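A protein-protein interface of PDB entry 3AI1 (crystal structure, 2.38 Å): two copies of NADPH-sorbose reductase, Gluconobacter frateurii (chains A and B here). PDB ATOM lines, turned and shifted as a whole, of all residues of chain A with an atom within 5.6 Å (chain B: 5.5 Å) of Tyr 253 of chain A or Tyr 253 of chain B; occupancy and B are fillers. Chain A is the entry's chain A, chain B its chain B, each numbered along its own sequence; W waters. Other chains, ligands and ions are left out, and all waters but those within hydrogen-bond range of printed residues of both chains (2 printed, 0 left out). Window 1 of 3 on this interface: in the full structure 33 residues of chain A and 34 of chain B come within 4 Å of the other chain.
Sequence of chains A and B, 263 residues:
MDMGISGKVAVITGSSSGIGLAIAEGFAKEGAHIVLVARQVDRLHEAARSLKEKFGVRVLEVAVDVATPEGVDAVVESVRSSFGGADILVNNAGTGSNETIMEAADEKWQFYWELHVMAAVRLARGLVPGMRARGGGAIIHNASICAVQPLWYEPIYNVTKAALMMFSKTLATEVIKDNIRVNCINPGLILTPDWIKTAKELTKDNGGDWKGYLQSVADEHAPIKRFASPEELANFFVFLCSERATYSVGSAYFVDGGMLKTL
Phe 236 of chain A touches Leu 240 of chain B, and with the chains exchanged Leu 240 of chain A touches Phe 236 of chain B.
Phe 236 of chain A touches Tyr 253 of chain B, and with the chains exchanged Tyr 253 of chain A touches Phe 236 of chain B.
Tyr 253 of chain A touches its own counterpart, Tyr 253 of chain B.
Tyr 253 of chain A touches Phe 254 of chain B, and with the chains exchanged Phe 254 of chain A touches Tyr 253 of chain B.
Positions printed for both chains: 183, 184, 185, 186, 187, 236, 240, 248, 249, 251, 252, 253, 254 and 255.
Of the 11 pairs that touch across the chains among the printed residues, 11 have their exchanged pair printed and touching as well.
Printed residues of chain B within 4 Å of Ser 251 of chain A: Phe 254 (3.5 Å).
Of the printed residues of chain B, Tyr 253 of chain A touches Phe 236, Tyr 253 and Phe 254.
Of the printed residues of chain A, Leu 240 of chain B touches Phe 236 (3.9 Å).
Ala 252 of chain B touches none of the printed residues of chain A.
Of the printed residues of chain A, Phe 254 of chain B touches Ser 251 and Tyr 253.
The nearest residue of chain B that does not touch Tyr 253 of chain A is Val 255 of chain B (4.7 Å).
The nearest printed residue of chain A that does not touch Leu 240 of chain B is Tyr 253 of chain A (7.0 Å).
Water W2 lies within hydrogen-bond range of the side-chain hydroxyl of Ser 251 of chain B (2.6 Å), the backbone NH of Val 249 of chain B (3.2 Å) and the backbone carbonyl oxygen of Phe 254 of chain A (3.3 Å).
Water W1 lies within hydrogen-bond range of the side-chain hydroxyl of Ser 251 of chain A, the backbone NH of Val 249 of chain A and the backbone carbonyl oxygen of Phe 254 of chain B.
ND2 of Asn 183 of chain A lies within hydrogen-bond range of O of Ser 248 of chain A (2.8 Å).
N of Cys 184 of chain A is in hydrogen-bond range of O of Ser 251 of chain A, at 2.8 Å.
N of Asn 186 of chain A sits at hydrogen-bond distance from O of Tyr 253 of chain A (2.8 Å).
The side-chain hydroxyl (OG) of Ser 248 of chain A lies within hydrogen-bond range of the side-chain hydroxyl (OH) of Tyr 253 of chain A.
The backbone NH of Cys 184 of chain B sits at hydrogen-bond distance from the backbone carbonyl oxygen of Ser 251 of chain B (3.1 Å).
OG of Ser 248 of chain B lies within hydrogen-bond range of OH of Tyr 253 of chain B (2.6 Å).
Among the printed residues, merely in contact across the chains: Tyr 253 of chain A with Tyr 253 of chain B (3.2 Å), Phe 236 of chain A with Ser 248 of chain B (3.4 Å), Phe 236 of chain A with Tyr 253 of chain B (3.5 Å), Tyr 253 of chain A with Phe 236 of chain B (3.5 Å), Ser 248 of chain A with Phe 236 of chain B (3.8 Å), Phe 236 of chain A with Leu 240 of chain B (3.9 Å) and Leu 240 of chain A with Phe 236 of chain B (3.9 Å).
The backbone carbonyl oxygen (O) of Phe 254 of chain B is in hydrogen-bond range of the side-chain hydroxyl (OG) of Ser 251 of chain A (3.5 Å).
OH of Tyr 253 of chain A lies within hydrogen-bond range of O of Phe 254 of chain B.
O of Phe 254 of chain A lies within hydrogen-bond range of OG of Ser 251 of chain B.
The backbone carbonyl oxygen (O) of Phe 254 of chain A lies within hydrogen-bond range of the side-chain hydroxyl (OH) of Tyr 253 of chain B (2.7 Å).
Of the 14 printed residues of chain A, 6 touch a printed residue of chain B.
Hydrophobic or aromatic side chains of chain A that line the printed part of chain B: Phe 236, Leu 240, Tyr 253 and Phe 254.
Of the 14 printed residues of chain B, 6 touch a printed residue of chain A.
Among the printed residues, no Asp or Glu carboxylate lies within 4 Å of a Lys or Arg side-chain nitrogen of the other chain.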
ATOM      1  N   ASN A 183      21.131  19.064  20.375  1.00  0.00           N
ATOM      2  CA  ASN A 183      20.230  18.320  19.530  1.00  0.00           C
ATOM      3  C   ASN A 183      19.010  19.139  19.179  1.00  0.00           C
ATOM      4  O   ASN A 183      18.752  20.183  19.775  1.00  0.00           O
ATOM      5  CB  ASN A 183      19.831  17.006  20.196  1.00  0.00           C
ATOM      6  CG  ASN A 183      20.994  16.053  20.336  1.00  0.00           C
ATOM      7  OD1 ASN A 183      21.489  15.513  19.351  1.00  0.00           O
ATOM      8  ND2 ASN A 183      21.436  15.841  21.567  1.00  0.00           N
ATOM      9  N   CYS A 184      18.265  18.645  18.202  1.00  0.00           N
ATOM     10  CA  CYS A 184      17.129  19.343  17.652  1.00  0.00           C
ATOM     11  C   CYS A 184      15.912  18.426  17.693  1.00  0.00           C
ATOM     12  O   CYS A 184      16.000  17.225  17.377  1.00  0.00           O
ATOM     13  CB  CYS A 184      17.450  19.753  16.217  1.00  0.00           C
ATOM     14  SG  CYS A 184      16.234  20.805  15.438  1.00  0.00           S
ATOM     15  N   ILE A 185      14.782  18.985  18.110  1.00  0.00           N
ATOM     16  CA  ILE A 185      13.513  18.265  18.059  1.00  0.00           C
ATOM     17  C   ILE A 185      12.576  18.940  17.067  1.00  0.00           C
ATOM     18  O   ILE A 185      12.460  20.169  17.024  1.00  0.00           O
ATOM     19  CB  ILE A 185      12.862  18.113  19.452  1.00  0.00           C
ATOM     20  CG1 ILE A 185      13.742  17.230  20.343  1.00  0.00           C
ATOM     21  CG2 ILE A 185      11.453  17.520  19.343  1.00  0.00           C
ATOM     22  CD1 ILE A 185      13.295  17.155  21.789  1.00  0.00           C
ATOM     23  N   ASN A 186      11.936  18.118  16.250  1.00  0.00           N
ATOM     24  CA  ASN A 186      11.017  18.596  15.240  1.00  0.00           C
ATOM     25  C   ASN A 186       9.635  18.002  15.462  1.00  0.00           C
ATOM     26  O   ASN A 186       9.347  16.885  15.012  1.00  0.00           O
ATOM     27  CB  ASN A 186      11.555  18.280  13.857  1.00  0.00           C
ATOM     28  CG  ASN A 186      12.856  18.988  13.579  1.00  0.00           C
ATOM     29  OD1 ASN A 186      13.891  18.362  13.416  1.00  0.00           O
ATOM     30  ND2 ASN A 186      12.813  20.307  13.555  1.00  0.00           N
ATOM     31  N   PRO A 187       8.786  18.741  16.195  1.00  0.00           N
ATOM     32  CA  PRO A 187       7.438  18.304  16.497  1.00  0.00           C
ATOM     33  C   PRO A 187       6.522  18.392  15.284  1.00  0.00           C
ATOM     34  O   PRO A 187       6.715  19.247  14.415  1.00  0.00           O
ATOM     35  CB  PRO A 187       6.983  19.288  17.578  1.00  0.00           C
ATOM     36  CG  PRO A 187       7.811  20.499  17.373  1.00  0.00           C
ATOM     37  CD  PRO A 187       9.133  19.992  16.895  1.00  0.00           C
ATOM     38  N   PHE A 236      10.270  13.697  25.370  1.00  0.00           N
ATOM     39  CA  PHE A 236      11.396  13.616  24.461  1.00  0.00           C
ATOM     40  C   PHE A 236      12.468  14.664  24.776  1.00  0.00           C
ATOM     41  O   PHE A 236      13.660  14.365  24.751  1.00  0.00           O
ATOM     42  CB  PHE A 236      10.910  13.752  23.021  1.00  0.00           C
ATOM     43  CG  PHE A 236      11.470  12.723  22.109  1.00  0.00           C
ATOM     44  CD1 PHE A 236      10.727  11.588  21.790  1.00  0.00           C
ATOM     45  CD2 PHE A 236      12.751  12.860  21.588  1.00  0.00           C
ATOM     46  CE1 PHE A 236      11.244  10.605  20.946  1.00  0.00           C
ATOM     47  CE2 PHE A 236      13.286  11.876  20.750  1.00  0.00           C
ATOM     48  CZ  PHE A 236      12.527  10.748  20.431  1.00  0.00           C
ATOM     49  N   LEU A 240      16.318  13.605  26.094  1.00  0.00           N
ATOM     50  CA  LEU A 240      17.427  14.069  25.269  1.00  0.00           C
ATOM     51  C   LEU A 240      18.385  15.012  26.003  1.00  0.00           C
ATOM     52  O   LEU A 240      19.513  15.253  25.546  1.00  0.00           O
ATOM     53  CB  LEU A 240      16.862  14.768  24.041  1.00  0.00           C
ATOM     54  CG  LEU A 240      17.354  14.364  22.660  1.00  0.00           C
ATOM     55  CD1 LEU A 240      17.118  12.873  22.389  1.00  0.00           C
ATOM     56  CD2 LEU A 240      16.622  15.226  21.639  1.00  0.00           C
ATOM     57  N   SER A 248      23.891  11.383  21.815  1.00  0.00           N
ATOM     58  CA  SER A 248      23.146  12.211  20.873  1.00  0.00           C
ATOM     59  C   SER A 248      23.810  13.571  20.708  1.00  0.00           C
ATOM     60  O   SER A 248      23.800  14.401  21.622  1.00  0.00           O
ATOM     61  CB  SER A 248      21.697  12.369  21.329  1.00  0.00           C
ATOM     62  OG  SER A 248      20.994  11.145  21.174  1.00  0.00           O
ATOM     63  N   VAL A 249      24.398  13.782  19.535  1.00  0.00           N
ATOM     64  CA  VAL A 249      25.108  15.022  19.229  1.00  0.00           C
ATOM     65  C   VAL A 249      24.784  15.466  17.799  1.00  0.00           C
ATOM     66  O   VAL A 249      25.091  14.753  16.844  1.00  0.00           O
ATOM     67  CB  VAL A 249      26.648  14.867  19.376  1.00  0.00           C
ATOM     68  CG1 VAL A 249      27.329  16.214  19.247  1.00  0.00           C
ATOM     69  CG2 VAL A 249      27.013  14.230  20.707  1.00  0.00           C
ATOM     70  N   SER A 251      21.883  15.782  16.264  1.00  0.00           N
ATOM     71  CA  SER A 251      20.828  15.059  15.580  1.00  0.00           C
ATOM     72  C   SER A 251      19.508  15.825  15.591  1.00  0.00           C
ATOM     73  O   SER A 251      19.278  16.702  16.436  1.00  0.00           O
ATOM     74  CB  SER A 251      20.649  13.665  16.172  1.00  0.00           C
ATOM     75  OG  SER A 251      21.805  12.877  15.977  1.00  0.00           O
ATOM     76  N   ALA A 252      18.659  15.492  14.627  1.00  0.00           N
ATOM     77  CA  ALA A 252      17.326  16.046  14.526  1.00  0.00           C
ATOM     78  C   ALA A 252      16.357  14.895  14.744  1.00  0.00           C
ATOM     79  O   ALA A 252      16.383  13.912  14.005  1.00  0.00           O
ATOM     80  CB  ALA A 252      17.118  16.682  13.158  1.00  0.00           C
ATOM     81  N   TYR A 253      15.528  15.023  15.778  1.00  0.00           N
ATOM     82  CA  TYR A 253      14.583  13.987  16.178  1.00  0.00           C
ATOM     83  C   TYR A 253      13.135  14.419  15.917  1.00  0.00           C
ATOM     84  O   TYR A 253      12.679  15.470  16.387  1.00  0.00           O
ATOM     85  CB  TYR A 253      14.783  13.623  17.655  1.00  0.00           C
ATOM     86  CG  TYR A 253      16.170  13.101  17.969  1.00  0.00           C
ATOM     87  CD1 TYR A 253      17.146  13.937  18.493  1.00  0.00           C
ATOM     88  CD2 TYR A 253      16.508  11.770  17.724  1.00  0.00           C
ATOM     89  CE1 TYR A 253      18.422  13.465  18.778  1.00  0.00           C
ATOM     90  CE2 TYR A 253      17.780  11.286  17.998  1.00  0.00           C
ATOM     91  CZ  TYR A 253      18.731  12.136  18.529  1.00  0.00           C
ATOM     92  OH  TYR A 253      19.991  11.660  18.797  1.00  0.00           O
ATOM     93  N   PHE A 254      12.425  13.597  15.158  1.00  0.00           N
ATOM     94  CA  PHE A 254      11.059  13.897  14.769  1.00  0.00           C
ATOM     95  C   PHE A 254      10.062  13.282  15.731  1.00  0.00           C
ATOM     96  O   PHE A 254      10.145  12.099  16.062  1.00  0.00           O
ATOM     97  CB  PHE A 254      10.797  13.451  13.328  1.00  0.00           C
ATOM     98  CG  PHE A 254      11.502  14.301  12.300  1.00  0.00           C
ATOM     99  CD1 PHE A 254      12.835  14.050  11.961  1.00  0.00           C
ATOM    100  CD2 PHE A 254      10.841  15.366  11.689  1.00  0.00           C
ATOM    101  CE1 PHE A 254      13.502  14.844  11.023  1.00  0.00           C
ATOM    102  CE2 PHE A 254      11.494  16.169  10.747  1.00  0.00           C
ATOM    103  CZ  PHE A 254      12.829  15.905  10.412  1.00  0.00           C
ATOM    104  N   VAL A 255       9.141  14.108  16.213  1.00  0.00           N
ATOM    105  CA  VAL A 255       8.032  13.627  17.029  1.00  0.00           C
ATOM    106  C   VAL A 255       6.782  14.124  16.320  1.00  0.00           C
ATOM    107  O   VAL A 255       6.276  15.211  16.613  1.00  0.00           O
ATOM    108  CB  VAL A 255       8.103  14.152  18.485  1.00  0.00           C
ATOM    109  CG1 VAL A 255       7.194  13.323  19.393  1.00  0.00           C
ATOM    110  CG2 VAL A 255       9.546  14.137  19.012  1.00  0.00           C
ATOM    111  N   ASN B 183       9.444   2.382  14.565  1.00  0.00           N
ATOM    112  CA  ASN B 183      10.540   3.320  14.365  1.00  0.00           C
ATOM    113  C   ASN B 183      11.848   2.628  14.043  1.00  0.00           C
ATOM    114  O   ASN B 183      11.932   1.403  14.012  1.00  0.00           O
ATOM    115  CB  ASN B 183      10.719   4.228  15.576  1.00  0.00           C
ATOM    116  CG  ASN B 183       9.532   5.127  15.799  1.00  0.00           C
ATOM    117  OD1 ASN B 183       9.336   6.102  15.076  1.00  0.00           O
ATOM    118  ND2 ASN B 183       8.726   4.805  16.805  1.00  0.00           N
ATOM    119  N   CYS B 184      12.869   3.448  13.824  1.00  0.00           N
ATOM    120  CA  CYS B 184      14.149   3.018  13.316  1.00  0.00           C
ATOM    121  C   CYS B 184      15.232   3.804  14.040  1.00  0.00           C
ATOM    122  O   CYS B 184      15.119   5.026  14.208  1.00  0.00           O
ATOM    123  CB  CYS B 184      14.199   3.303  11.817  1.00  0.00           C
ATOM    124  SG  CYS B 184      15.768   2.968  11.021  1.00  0.00           S
ATOM    125  N   ILE B 185      16.264   3.087  14.480  1.00  0.00           N
ATOM    126  CA  ILE B 185      17.414   3.665  15.167  1.00  0.00           C
ATOM    127  C   ILE B 185      18.680   3.429  14.336  1.00  0.00           C
ATOM    128  O   ILE B 185      18.947   2.308  13.887  1.00  0.00           O
ATOM    129  CB  ILE B 185      17.574   3.084  16.601  1.00  0.00           C
ATOM    130  CG1 ILE B 185      16.370   3.460  17.460  1.00  0.00           C
ATOM    131  CG2 ILE B 185      18.869   3.571  17.263  1.00  0.00           C
ATOM    132  CD1 ILE B 185      16.424   2.928  18.900  1.00  0.00           C
ATOM    133  N   ASN B 186      19.439   4.499  14.120  1.00  0.00           N
ATOM    134  CA  ASN B 186      20.654   4.437  13.322  1.00  0.00           C
ATOM    135  C   ASN B 186      21.883   4.750  14.169  1.00  0.00           C
ATOM    136  O   ASN B 186      22.248   5.919  14.336  1.00  0.00           O
ATOM    137  CB  ASN B 186      20.553   5.385  12.129  1.00  0.00           C
ATOM    138  CG  ASN B 186      19.430   5.010  11.188  1.00  0.00           C
ATOM    139  OD1 ASN B 186      19.463   3.965  10.538  1.00  0.00           O
ATOM    140  ND2 ASN B 186      18.421   5.855  11.120  1.00  0.00           N
ATOM    141  N   PRO B 187      22.519   3.702  14.725  1.00  0.00           N
ATOM    142  CA  PRO B 187      23.687   3.887  15.574  1.00  0.00           C
ATOM    143  C   PRO B 187      24.930   4.256  14.774  1.00  0.00           C
ATOM    144  O   PRO B 187      25.065   3.860  13.623  1.00  0.00           O
ATOM    145  CB  PRO B 187      23.864   2.513  16.220  1.00  0.00           C
ATOM    146  CG  PRO B 187      23.329   1.567  15.217  1.00  0.00           C
ATOM    147  CD  PRO B 187      22.165   2.277  14.588  1.00  0.00           C
ATOM    148  N   PHE B 236      18.217   4.359  24.294  1.00  0.00           N
ATOM    149  CA  PHE B 236      17.345   4.891  23.252  1.00  0.00           C
ATOM    150  C   PHE B 236      16.289   3.891  22.778  1.00  0.00           C
ATOM    151  O   PHE B 236      15.151   4.279  22.509  1.00  0.00           O
ATOM    152  CB  PHE B 236      18.162   5.414  22.062  1.00  0.00           C
ATOM    153  CG  PHE B 236      17.654   6.714  21.525  1.00  0.00           C
ATOM    154  CD1 PHE B 236      18.285   7.911  21.870  1.00  0.00           C
ATOM    155  CD2 PHE B 236      16.521   6.756  20.718  1.00  0.00           C
ATOM    156  CE1 PHE B 236      17.805   9.129  21.401  1.00  0.00           C
ATOM    157  CE2 PHE B 236      16.025   7.964  20.248  1.00  0.00           C
ATOM    158  CZ  PHE B 236      16.673   9.157  20.588  1.00  0.00           C
ATOM    159  N   LEU B 240      12.158   4.519  23.285  1.00  0.00           N
ATOM    160  CA  LEU B 240      11.321   4.478  22.084  1.00  0.00           C
ATOM    161  C   LEU B 240      10.257   3.378  22.102  1.00  0.00           C
ATOM    162  O   LEU B 240       9.270   3.447  21.364  1.00  0.00           O
ATOM    163  CB  LEU B 240      12.195   4.324  20.847  1.00  0.00           C
ATOM    164  CG  LEU B 240      12.374   5.489  19.873  1.00  0.00           C
ATOM    165  CD1 LEU B 240      12.467   6.861  20.552  1.00  0.00           C
ATOM    166  CD2 LEU B 240      13.601   5.219  19.042  1.00  0.00           C
ATOM    167  N   SER B 248       5.982   8.824  18.560  1.00  0.00           N
ATOM    168  CA  SER B 248       7.042   8.459  17.624  1.00  0.00           C
ATOM    169  C   SER B 248       6.541   7.404  16.658  1.00  0.00           C
ATOM    170  O   SER B 248       6.305   6.264  17.045  1.00  0.00           O
ATOM    171  CB  SER B 248       8.269   7.958  18.375  1.00  0.00           C
ATOM    172  OG  SER B 248       8.961   9.047  18.964  1.00  0.00           O
ATOM    173  N   VAL B 249       6.360   7.806  15.401  1.00  0.00           N
ATOM    174  CA  VAL B 249       5.834   6.927  14.364  1.00  0.00           C
ATOM    175  C   VAL B 249       6.587   7.172  13.058  1.00  0.00           C
ATOM    176  O   VAL B 249       6.680   8.315  12.596  1.00  0.00           O
ATOM    177  CB  VAL B 249       4.319   7.163  14.130  1.00  0.00           C
ATOM    178  CG1 VAL B 249       3.799   6.300  12.973  1.00  0.00           C
ATOM    179  CG2 VAL B 249       3.512   6.903  15.402  1.00  0.00           C
ATOM    180  N   SER B 251       9.703   7.237  12.274  1.00  0.00           N
ATOM    181  CA  SER B 251      10.850   8.128  12.332  1.00  0.00           C
ATOM    182  C   SER B 251      12.170   7.368  12.318  1.00  0.00           C
ATOM    183  O   SER B 251      12.204   6.152  12.507  1.00  0.00           O
ATOM    184  CB  SER B 251      10.751   9.054  13.539  1.00  0.00           C
ATOM    185  OG  SER B 251       9.640   9.926  13.400  1.00  0.00           O
ATOM    186  N   ALA B 252      13.248   8.093  12.044  1.00  0.00           N
ATOM    187  CA  ALA B 252      14.581   7.520  12.020  1.00  0.00           C
ATOM    188  C   ALA B 252      15.407   8.319  12.999  1.00  0.00           C
ATOM    189  O   ALA B 252      15.658   9.513  12.795  1.00  0.00           O
ATOM    190  CB  ALA B 252      15.174   7.594  10.628  1.00  0.00           C
ATOM    191  N   TYR B 253      15.796   7.665  14.083  1.00  0.00           N
ATOM    192  CA  TYR B 253      16.527   8.323  15.139  1.00  0.00           C
ATOM    193  C   TYR B 253      18.001   7.953  15.081  1.00  0.00           C
ATOM    194  O   TYR B 253      18.370   6.776  15.067  1.00  0.00           O
ATOM    195  CB  TYR B 253      15.914   7.993  16.497  1.00  0.00           C
ATOM    196  CG  TYR B 253      14.461   8.420  16.624  1.00  0.00           C
ATOM    197  CD1 TYR B 253      13.430   7.502  16.461  1.00  0.00           C
ATOM    198  CD2 TYR B 253      14.126   9.745  16.898  1.00  0.00           C
ATOM    199  CE1 TYR B 253      12.105   7.884  16.583  1.00  0.00           C
ATOM    200  CE2 TYR B 253      12.801  10.142  17.012  1.00  0.00           C
ATOM    201  CZ  TYR B 253      11.800   9.206  16.856  1.00  0.00           C
ATOM    202  OH  TYR B 253      10.493   9.601  16.961  1.00  0.00           O
ATOM    203  N   PHE B 254      18.833   8.981  15.023  1.00  0.00           N
ATOM    204  CA  PHE B 254      20.267   8.816  14.921  1.00  0.00           C
ATOM    205  C   PHE B 254      20.920   8.887  16.294  1.00  0.00           C
ATOM    206  O   PHE B 254      20.651   9.799  17.077  1.00  0.00           O
ATOM    207  CB  PHE B 254      20.839   9.866  13.968  1.00  0.00           C
ATOM    208  CG  PHE B 254      20.609   9.544  12.517  1.00  0.00           C
ATOM    209  CD1 PHE B 254      19.397   9.848  11.902  1.00  0.00           C
ATOM    210  CD2 PHE B 254      21.599   8.912  11.767  1.00  0.00           C
ATOM    211  CE1 PHE B 254      19.178   9.529  10.563  1.00  0.00           C
ATOM    212  CE2 PHE B 254      21.392   8.593  10.424  1.00  0.00           C
ATOM    213  CZ  PHE B 254      20.180   8.903   9.823  1.00  0.00           C
ATOM    214  N   VAL B 255      21.736   7.885  16.604  1.00  0.00           N
ATOM    215  CA  VAL B 255      22.556   7.904  17.817  1.00  0.00           C
ATOM    216  C   VAL B 255      23.997   7.667  17.377  1.00  0.00           C
ATOM    217  O   VAL B 255      24.469   6.522  17.311  1.00  0.00           O
ATOM    218  CB  VAL B 255      22.102   6.856  18.854  1.00  0.00           C
ATOM    219  CG1 VAL B 255      22.849   7.052  20.170  1.00  0.00           C
ATOM    220  CG2 VAL B 255      20.599   6.948  19.090  1.00  0.00           C
HETATM  221  O   HOH W   1      23.605  11.468  17.416  1.00  0.00           O
HETATM  222  O   HOH W   2       7.513  10.676  14.654  1.00  0.00           O
